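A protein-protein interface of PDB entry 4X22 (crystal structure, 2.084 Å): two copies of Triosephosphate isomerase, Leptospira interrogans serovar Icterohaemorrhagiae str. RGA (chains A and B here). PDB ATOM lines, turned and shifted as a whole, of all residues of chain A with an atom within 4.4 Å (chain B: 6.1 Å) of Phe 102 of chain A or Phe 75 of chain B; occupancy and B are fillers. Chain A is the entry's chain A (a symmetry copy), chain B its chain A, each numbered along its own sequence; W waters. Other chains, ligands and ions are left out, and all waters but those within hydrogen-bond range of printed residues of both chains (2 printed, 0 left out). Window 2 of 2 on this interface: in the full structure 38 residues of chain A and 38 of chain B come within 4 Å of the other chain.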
ATOM      1  N   LYS A  11      23.907  21.408 -17.313  1.00  0.00           N
ATOM      2  CA  LYS A  11      22.477  21.645 -17.462  1.00  0.00           C
ATOM      3  C   LYS A  11      22.176  22.111 -18.885  1.00  0.00           C
ATOM      4  O   LYS A  11      22.705  21.530 -19.887  1.00  0.00           O
ATOM      5  CB  LYS A  11      21.935  22.549 -16.343  1.00  0.00           C
ATOM      6  CG  LYS A  11      22.355  22.106 -14.953  1.00  0.00           C
ATOM      7  CD  LYS A  11      21.593  22.907 -13.862  1.00  0.00           C
ATOM      8  CE  LYS A  11      21.938  22.345 -12.490  1.00  0.00           C
ATOM      9  NZ  LYS A  11      21.129  23.017 -11.422  1.00  0.00           N
ATOM     10  N   MET A  12      21.328  23.114 -19.013  1.00  0.00           N
ATOM     11  CA  MET A  12      20.977  23.674 -20.322  1.00  0.00           C
ATOM     12  C   MET A  12      21.554  25.117 -20.360  1.00  0.00           C
ATOM     13  O   MET A  12      21.039  25.993 -21.043  1.00  0.00           O
ATOM     14  CB  MET A  12      19.469  23.651 -20.449  1.00  0.00           C
ATOM     15  CG  MET A  12      18.932  23.928 -21.842  1.00  0.00           C
ATOM     16  SD  MET A  12      17.152  23.896 -22.014  1.00  0.00           S
ATOM     17  CE  MET A  12      16.823  25.470 -21.209  1.00  0.00           C
ATOM     18  N   GLU A  98      15.439  18.784 -11.453  1.00  0.00           N
ATOM     19  CA  GLU A  98      14.792  19.594 -12.527  1.00  0.00           C
ATOM     20  C   GLU A  98      13.929  18.752 -13.397  1.00  0.00           C
ATOM     21  O   GLU A  98      12.886  19.279 -13.895  1.00  0.00           O
ATOM     22  CB  GLU A  98      15.768  20.428 -13.375  1.00  0.00           C
ATOM     23  CG  GLU A  98      16.415  21.462 -12.442  1.00  0.00           C
ATOM     24  CD  GLU A  98      17.840  21.901 -12.786  1.00  0.00           C
ATOM     25  OE1 GLU A  98      18.406  21.535 -13.858  1.00  0.00           O
ATOM     26  OE2 GLU A  98      18.427  22.634 -11.944  1.00  0.00           O
ATOM     27  N   ARG A  99      14.320  17.463 -13.590  1.00  0.00           N
ATOM     28  CA  ARG A  99      13.488  16.533 -14.373  1.00  0.00           C
ATOM     29  C   ARG A  99      12.260  16.038 -13.601  1.00  0.00           C
ATOM     30  O   ARG A  99      11.120  15.963 -14.170  1.00  0.00           O
ATOM     31  CB  ARG A  99      14.319  15.367 -14.945  1.00  0.00           C
ATOM     32  CG  ARG A  99      15.409  15.899 -15.885  1.00  0.00           C
ATOM     33  CD  ARG A  99      15.891  14.806 -16.874  1.00  0.00           C
ATOM     34  NE  ARG A  99      14.795  14.508 -17.809  1.00  0.00           N
ATOM     35  CZ  ARG A  99      14.409  15.309 -18.813  1.00  0.00           C
ATOM     36  NH1 ARG A  99      15.013  16.469 -19.074  1.00  0.00           N
ATOM     37  NH2 ARG A  99      13.415  14.951 -19.591  1.00  0.00           N
ATOM     38  N   ARG A 100      12.435  15.773 -12.308  1.00  0.00           N
ATOM     39  CA  ARG A 100      11.297  15.376 -11.480  1.00  0.00           C
ATOM     40  C   ARG A 100      10.285  16.550 -11.421  1.00  0.00           C
ATOM     41  O   ARG A 100       9.094  16.355 -11.635  1.00  0.00           O
ATOM     42  CB  ARG A 100      11.701  14.924 -10.083  1.00  0.00           C
ATOM     43  CG  ARG A 100      12.706  13.824 -10.071  1.00  0.00           C
ATOM     44  CD  ARG A 100      13.077  13.556  -8.635  1.00  0.00           C
ATOM     45  NE  ARG A 100      14.000  12.457  -8.439  1.00  0.00           N
ATOM     46  CZ  ARG A 100      13.631  11.235  -8.147  1.00  0.00           C
ATOM     47  NH1 ARG A 100      12.349  10.890  -8.148  1.00  0.00           N
ATOM     48  NH2 ARG A 100      14.551  10.310  -7.960  1.00  0.00           N
ATOM     49  N   GLN A 101      10.780  17.749 -11.203  1.00  0.00           N
ATOM     50  CA  GLN A 101       9.908  18.926 -11.046  1.00  0.00           C
ATOM     51  C   GLN A 101       9.326  19.497 -12.366  1.00  0.00           C
ATOM     52  O   GLN A 101       8.122  19.766 -12.463  1.00  0.00           O
ATOM     53  CB  GLN A 101      10.651  20.006 -10.293  1.00  0.00           C
ATOM     54  CG  GLN A 101       9.873  21.300 -10.357  1.00  0.00           C
ATOM     55  CD  GLN A 101      10.394  22.414  -9.468  1.00  0.00           C
ATOM     56  OE1 GLN A 101      11.523  22.358  -8.948  1.00  0.00           O
ATOM     57  NE2 GLN A 101       9.553  23.458  -9.291  1.00  0.00           N
ATOM     58  N   PHE A 102      10.165  19.728 -13.376  1.00  0.00           N
ATOM     59  CA  PHE A 102       9.714  20.383 -14.605  1.00  0.00           C
ATOM     60  C   PHE A 102       9.284  19.449 -15.744  1.00  0.00           C
ATOM     61  O   PHE A 102       8.596  19.901 -16.656  1.00  0.00           O
ATOM     62  CB  PHE A 102      10.736  21.404 -15.098  1.00  0.00           C
ATOM     63  CG  PHE A 102      11.033  22.482 -14.085  1.00  0.00           C
ATOM     64  CD1 PHE A 102      10.098  23.511 -13.828  1.00  0.00           C
ATOM     65  CD2 PHE A 102      12.222  22.463 -13.390  1.00  0.00           C
ATOM     66  CE1 PHE A 102      10.391  24.495 -12.892  1.00  0.00           C
ATOM     67  CE2 PHE A 102      12.506  23.444 -12.423  1.00  0.00           C
ATOM     68  CZ  PHE A 102      11.598  24.455 -12.182  1.00  0.00           C
ATOM     69  N   LEU A 103       9.695  18.177 -15.703  1.00  0.00           N
ATOM     70  CA  LEU A 103       9.374  17.205 -16.728  1.00  0.00           C
ATOM     71  C   LEU A 103       8.528  16.015 -16.126  1.00  0.00           C
ATOM     72  O   LEU A 103       8.224  15.039 -16.785  1.00  0.00           O
ATOM     73  CB  LEU A 103      10.639  16.748 -17.466  1.00  0.00           C
ATOM     74  CG  LEU A 103      11.370  17.668 -18.488  1.00  0.00           C
ATOM     75  CD1 LEU A 103      10.355  18.234 -19.448  1.00  0.00           C
ATOM     76  CD2 LEU A 103      12.152  18.803 -17.824  1.00  0.00           C
ATOM     77  N   GLY A 104       8.099  16.166 -14.886  1.00  0.00           N
ATOM     78  CA  GLY A 104       7.184  15.261 -14.250  1.00  0.00           C
ATOM     79  C   GLY A 104       7.726  13.823 -14.161  1.00  0.00           C
ATOM     80  O   GLY A 104       6.959  12.912 -14.136  1.00  0.00           O
ATOM     81  N   TYR B  68      12.660  22.617 -24.916  1.00  0.00           N
ATOM     82  CA  TYR B  68      12.000  23.142 -23.718  1.00  0.00           C
ATOM     83  C   TYR B  68      11.754  24.634 -23.952  1.00  0.00           C
ATOM     84  O   TYR B  68      12.441  25.254 -24.762  1.00  0.00           O
ATOM     85  CB  TYR B  68      12.875  22.938 -22.469  1.00  0.00           C
ATOM     86  CG  TYR B  68      12.129  23.164 -21.194  1.00  0.00           C
ATOM     87  CD1 TYR B  68      11.163  22.279 -20.771  1.00  0.00           C
ATOM     88  CD2 TYR B  68      12.347  24.334 -20.422  1.00  0.00           C
ATOM     89  CE1 TYR B  68      10.480  22.484 -19.589  1.00  0.00           C
ATOM     90  CE2 TYR B  68      11.650  24.572 -19.261  1.00  0.00           C
ATOM     91  CZ  TYR B  68      10.728  23.645 -18.838  1.00  0.00           C
ATOM     92  OH  TYR B  68      10.050  23.882 -17.708  1.00  0.00           O
ATOM     93  N   HIS B  69      10.799  25.210 -23.225  1.00  0.00           N
ATOM     94  CA  HIS B  69      10.409  26.600 -23.457  1.00  0.00           C
ATOM     95  C   HIS B  69      11.249  27.565 -22.624  1.00  0.00           C
ATOM     96  O   HIS B  69      10.727  28.246 -21.745  1.00  0.00           O
ATOM     97  CB  HIS B  69       8.922  26.800 -23.161  1.00  0.00           C
ATOM     98  CG  HIS B  69       8.438  26.146 -21.887  1.00  0.00           C
ATOM     99  ND1 HIS B  69       8.610  26.714 -20.639  1.00  0.00           N
ATOM    100  CD2 HIS B  69       7.727  25.008 -21.676  1.00  0.00           C
ATOM    101  CE1 HIS B  69       8.065  25.933 -19.713  1.00  0.00           C
ATOM    102  NE2 HIS B  69       7.531  24.887 -20.309  1.00  0.00           N
ATOM    103  N   SER B  70      12.561  27.613 -22.880  1.00  0.00           N
ATOM    104  CA  SER B  70      13.443  28.527 -22.174  1.00  0.00           C
ATOM    105  C   SER B  70      14.717  28.762 -22.948  1.00  0.00           C
ATOM    106  O   SER B  70      15.182  27.882 -23.685  1.00  0.00           O
ATOM    107  CB  SER B  70      13.768  27.928 -20.795  1.00  0.00           C
ATOM    108  OG  SER B  70      14.680  28.750 -20.082  1.00  0.00           O
ATOM    109  N   GLY B  71      15.277  29.961 -22.816  1.00  0.00           N
ATOM    110  CA  GLY B  71      16.667  30.193 -23.178  1.00  0.00           C
ATOM    111  C   GLY B  71      17.578  29.475 -22.194  1.00  0.00           C
ATOM    112  O   GLY B  71      17.101  28.732 -21.316  1.00  0.00           O
ATOM    113  N   ALA B  73      19.471  27.990 -19.358  1.00  0.00           N
ATOM    114  CA  ALA B  73      19.050  28.031 -17.993  1.00  0.00           C
ATOM    115  C   ALA B  73      19.215  26.630 -17.414  1.00  0.00           C
ATOM    116  O   ALA B  73      19.653  25.658 -18.102  1.00  0.00           O
ATOM    117  CB  ALA B  73      17.592  28.495 -17.856  1.00  0.00           C
ATOM    118  N   ALA B  74      18.818  26.537 -16.163  1.00  0.00           N
ATOM    119  CA  ALA B  74      18.981  25.347 -15.313  1.00  0.00           C
ATOM    120  C   ALA B  74      17.875  24.284 -15.533  1.00  0.00           C
ATOM    121  O   ALA B  74      16.928  24.169 -14.750  1.00  0.00           O
ATOM    122  CB  ALA B  74      19.040  25.820 -13.858  1.00  0.00           C
ATOM    123  N   PHE B  75      17.891  23.595 -16.697  1.00  0.00           N
ATOM    124  CA  PHE B  75      16.882  22.544 -16.972  1.00  0.00           C
ATOM    125  C   PHE B  75      17.575  21.279 -17.463  1.00  0.00           C
ATOM    126  O   PHE B  75      17.673  21.039 -18.697  1.00  0.00           O
ATOM    127  CB  PHE B  75      15.777  23.005 -17.947  1.00  0.00           C
ATOM    128  CG  PHE B  75      14.907  24.112 -17.405  1.00  0.00           C
ATOM    129  CD1 PHE B  75      13.880  23.845 -16.526  1.00  0.00           C
ATOM    130  CD2 PHE B  75      15.133  25.429 -17.778  1.00  0.00           C
ATOM    131  CE1 PHE B  75      13.114  24.884 -15.970  1.00  0.00           C
ATOM    132  CE2 PHE B  75      14.370  26.468 -17.267  1.00  0.00           C
ATOM    133  CZ  PHE B  75      13.358  26.213 -16.357  1.00  0.00           C
ATOM    134  N   THR B  76      18.025  20.462 -16.505  1.00  0.00           N
ATOM    135  CA  THR B  76      18.829  19.290 -16.797  1.00  0.00           C
ATOM    136  C   THR B  76      18.101  18.395 -17.741  1.00  0.00           C
ATOM    137  O   THR B  76      16.868  18.151 -17.575  1.00  0.00           O
ATOM    138  CB  THR B  76      19.209  18.549 -15.497  1.00  0.00           C
ATOM    139  OG1 THR B  76      20.042  19.431 -14.747  1.00  0.00           O
ATOM    140  CG2 THR B  76      19.930  17.266 -15.756  1.00  0.00           C
ATOM    141  N   GLY B  77      18.803  17.980 -18.807  1.00  0.00           N
ATOM    142  CA  GLY B  77      18.221  17.082 -19.807  1.00  0.00           C
ATOM    143  C   GLY B  77      17.507  17.701 -20.986  1.00  0.00           C
ATOM    144  O   GLY B  77      17.144  16.977 -21.941  1.00  0.00           O
ATOM    145  N   GLU B  78      17.292  19.018 -20.937  1.00  0.00           N
ATOM    146  CA  GLU B  78      16.469  19.707 -21.937  1.00  0.00           C
ATOM    147  C   GLU B  78      17.391  20.422 -22.925  1.00  0.00           C
ATOM    148  O   GLU B  78      18.514  20.743 -22.612  1.00  0.00           O
ATOM    149  CB  GLU B  78      15.496  20.716 -21.309  1.00  0.00           C
ATOM    150  CG  GLU B  78      14.384  20.023 -20.506  1.00  0.00           C
ATOM    151  CD  GLU B  78      13.567  19.044 -21.397  1.00  0.00           C
ATOM    152  OE1 GLU B  78      12.868  19.532 -22.303  1.00  0.00           O
ATOM    153  OE2 GLU B  78      13.652  17.816 -21.184  1.00  0.00           O
ATOM    154  N   THR B  79      16.853  20.676 -24.087  1.00  0.00           N
ATOM    155  CA  THR B  79      17.526  21.438 -25.124  1.00  0.00           C
ATOM    156  C   THR B  79      16.826  22.821 -25.301  1.00  0.00           C
ATOM    157  O   THR B  79      15.602  22.937 -25.363  1.00  0.00           O
ATOM    158  CB  THR B  79      17.399  20.673 -26.459  1.00  0.00           C
ATOM    159  OG1 THR B  79      18.037  19.378 -26.368  1.00  0.00           O
ATOM    160  CG2 THR B  79      18.043  21.422 -27.606  1.00  0.00           C
ATOM    161  N   PHE B 109       1.461  21.852 -21.899  1.00  0.00           N
ATOM    162  CA  PHE B 109       2.936  21.864 -22.031  1.00  0.00           C
ATOM    163  C   PHE B 109       3.284  22.141 -23.499  1.00  0.00           C
ATOM    164  O   PHE B 109       4.098  22.988 -23.774  1.00  0.00           O
ATOM    165  CB  PHE B 109       3.469  20.519 -21.491  1.00  0.00           C
ATOM    166  CG  PHE B 109       4.970  20.421 -21.388  1.00  0.00           C
ATOM    167  CD1 PHE B 109       5.734  21.498 -21.018  1.00  0.00           C
ATOM    168  CD2 PHE B 109       5.596  19.210 -21.649  1.00  0.00           C
ATOM    169  CE1 PHE B 109       7.120  21.382 -20.891  1.00  0.00           C
ATOM    170  CE2 PHE B 109       6.989  19.047 -21.539  1.00  0.00           C
ATOM    171  CZ  PHE B 109       7.747  20.145 -21.140  1.00  0.00           C
HETATM  172  O   HOH W   1      20.775  20.006 -21.457  1.00  0.00           O
HETATM  173  O   HOH W   2       7.968  22.551 -16.956  1.00  0.00           O
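N of Ala 73 of chain B is in hydrogen-bond range of O of Met 12 of chain A. OG1 of Thr 76 of chain B is in hydrogen-bond range of OE1 of Glu 98 of chain A, 2.8 Å away. The backbone carbonyl oxygen (O) of Thr 76 of chain B lies within hydrogen-bond range of the guanidinium group (NH1) of Arg 99 of chain A (2.9 Å). The guanidinium group (NH1) of Arg 99 of chain A is in salt-bridge range of the side-chain carboxylate (OE2) of Glu 78 of chain B, 2.8 Å away. The side-chain sulfur (SD) of Met 12 of chain A sits close to the backbone carbonyl oxygen (O) of Glu 78 of chain B, 3.5 Å away. The side-chain carboxylate (OE1) of Glu 98 of chain A sits close to the backbone carbonyl oxygen (O) of Ala 74 of chain B (3.1 Å).
Of the 12 printed residues of chain B, 11 touch a printed residue of chain A. Of the 9 printed residues of chain A, 6 touch a printed residue of chain B. Hydrophobic or aromatic side chains of chain A within 4 Å of the printed part of chain B: Met 12, Phe 102 and Leu 103. Along chain A the printed residues that touch a printed residue of chain B span positions 11 to 103. Among the printed residues, Asp or Glu carboxylates within 4 Å of a Lys or Arg side-chain nitrogen of the other chain: Arg 99 of chain A with Glu 78 of chain B.
Phe 102 of chain A touches just these residues of chain B: Tyr 68 and Phe 75. Of chain A, only Met 12 (3.6 Å), Glu 98 (3.5 Å) and Phe 102 (3.6 Å) come within 4 Å of Phe 75 of chain B. Of the printed residues of chain A, Tyr 68 of chain B touches Phe 102. Of the printed residues of chain A, Ala 73 of chain B touches Met 12 (3.0 Å). Arg 100 of chain A touches none of the printed residues of chain B. Gly 104 of chain A touches none of the printed residues of chain B. The nearest residue of chain A that does not touch Phe 75 of chain B is Lys 11 of chain A (4.2 Å). The nearest printed residue of chain B that does not touch Arg 99 of chain A is Phe 75 of chain B (5.3 Å).
No position is printed for both chains. Of the 18 pairs that touch across the chains among the printed residues, none has its exchanged pair printed and touching as well.
Water W2 bridges OH of Tyr 68 of chain B (2.6 Å) and O of Phe 102 of chain A (2.7 Å). Water W1 bridges the backbone carbonyl oxygen of Glu 78 of chain B and the backbone carbonyl oxygen of Lys 11 of chain A.
O of Thr 79 of chain B lies within hydrogen-bond range of N of Tyr 68 of chain B, 3.0 Å away. The side-chain amino group (NZ) of Lys 11 of chain A lies within salt-bridge range of the side-chain carboxylate (OE2) of Glu 98 of chain A. The backbone carbonyl oxygen of Arg 99 of chain A lies within hydrogen-bond range of the backbone NH of Gly 104 of chain A, 3.1 Å away.
Among the printed residues, merely in contact across the chains: Met 12 of chain A with Gly 71 of chain B (3.3 Å), Arg 99 of chain A with Gly 77 of chain B (3.3 Å), Met 12 of chain A with Thr 79 of chain B (3.5 Å), Leu 103 of chain A with Glu 78 of chain B (3.5 Å), Lys 11 of chain A with Thr 76 of chain B (3.5 Å), Glu 98 of chain A with Phe 75 of chain B (3.5 Å), Met 12 of chain A with Phe 75 of chain B (3.6 Å), Phe 102 of chain A with Phe 75 of chain B (3.6 Å), Leu 103 of chain A with Phe 109 of chain B (3.6 Å), Phe 102 of chain A with Tyr 68 of chain B (3.7 Å), Met 12 of chain A with Ser 70 of chain B (3.8 Å) and Lys 11 of chain A with Ala 74 of chain B (3.9 Å).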
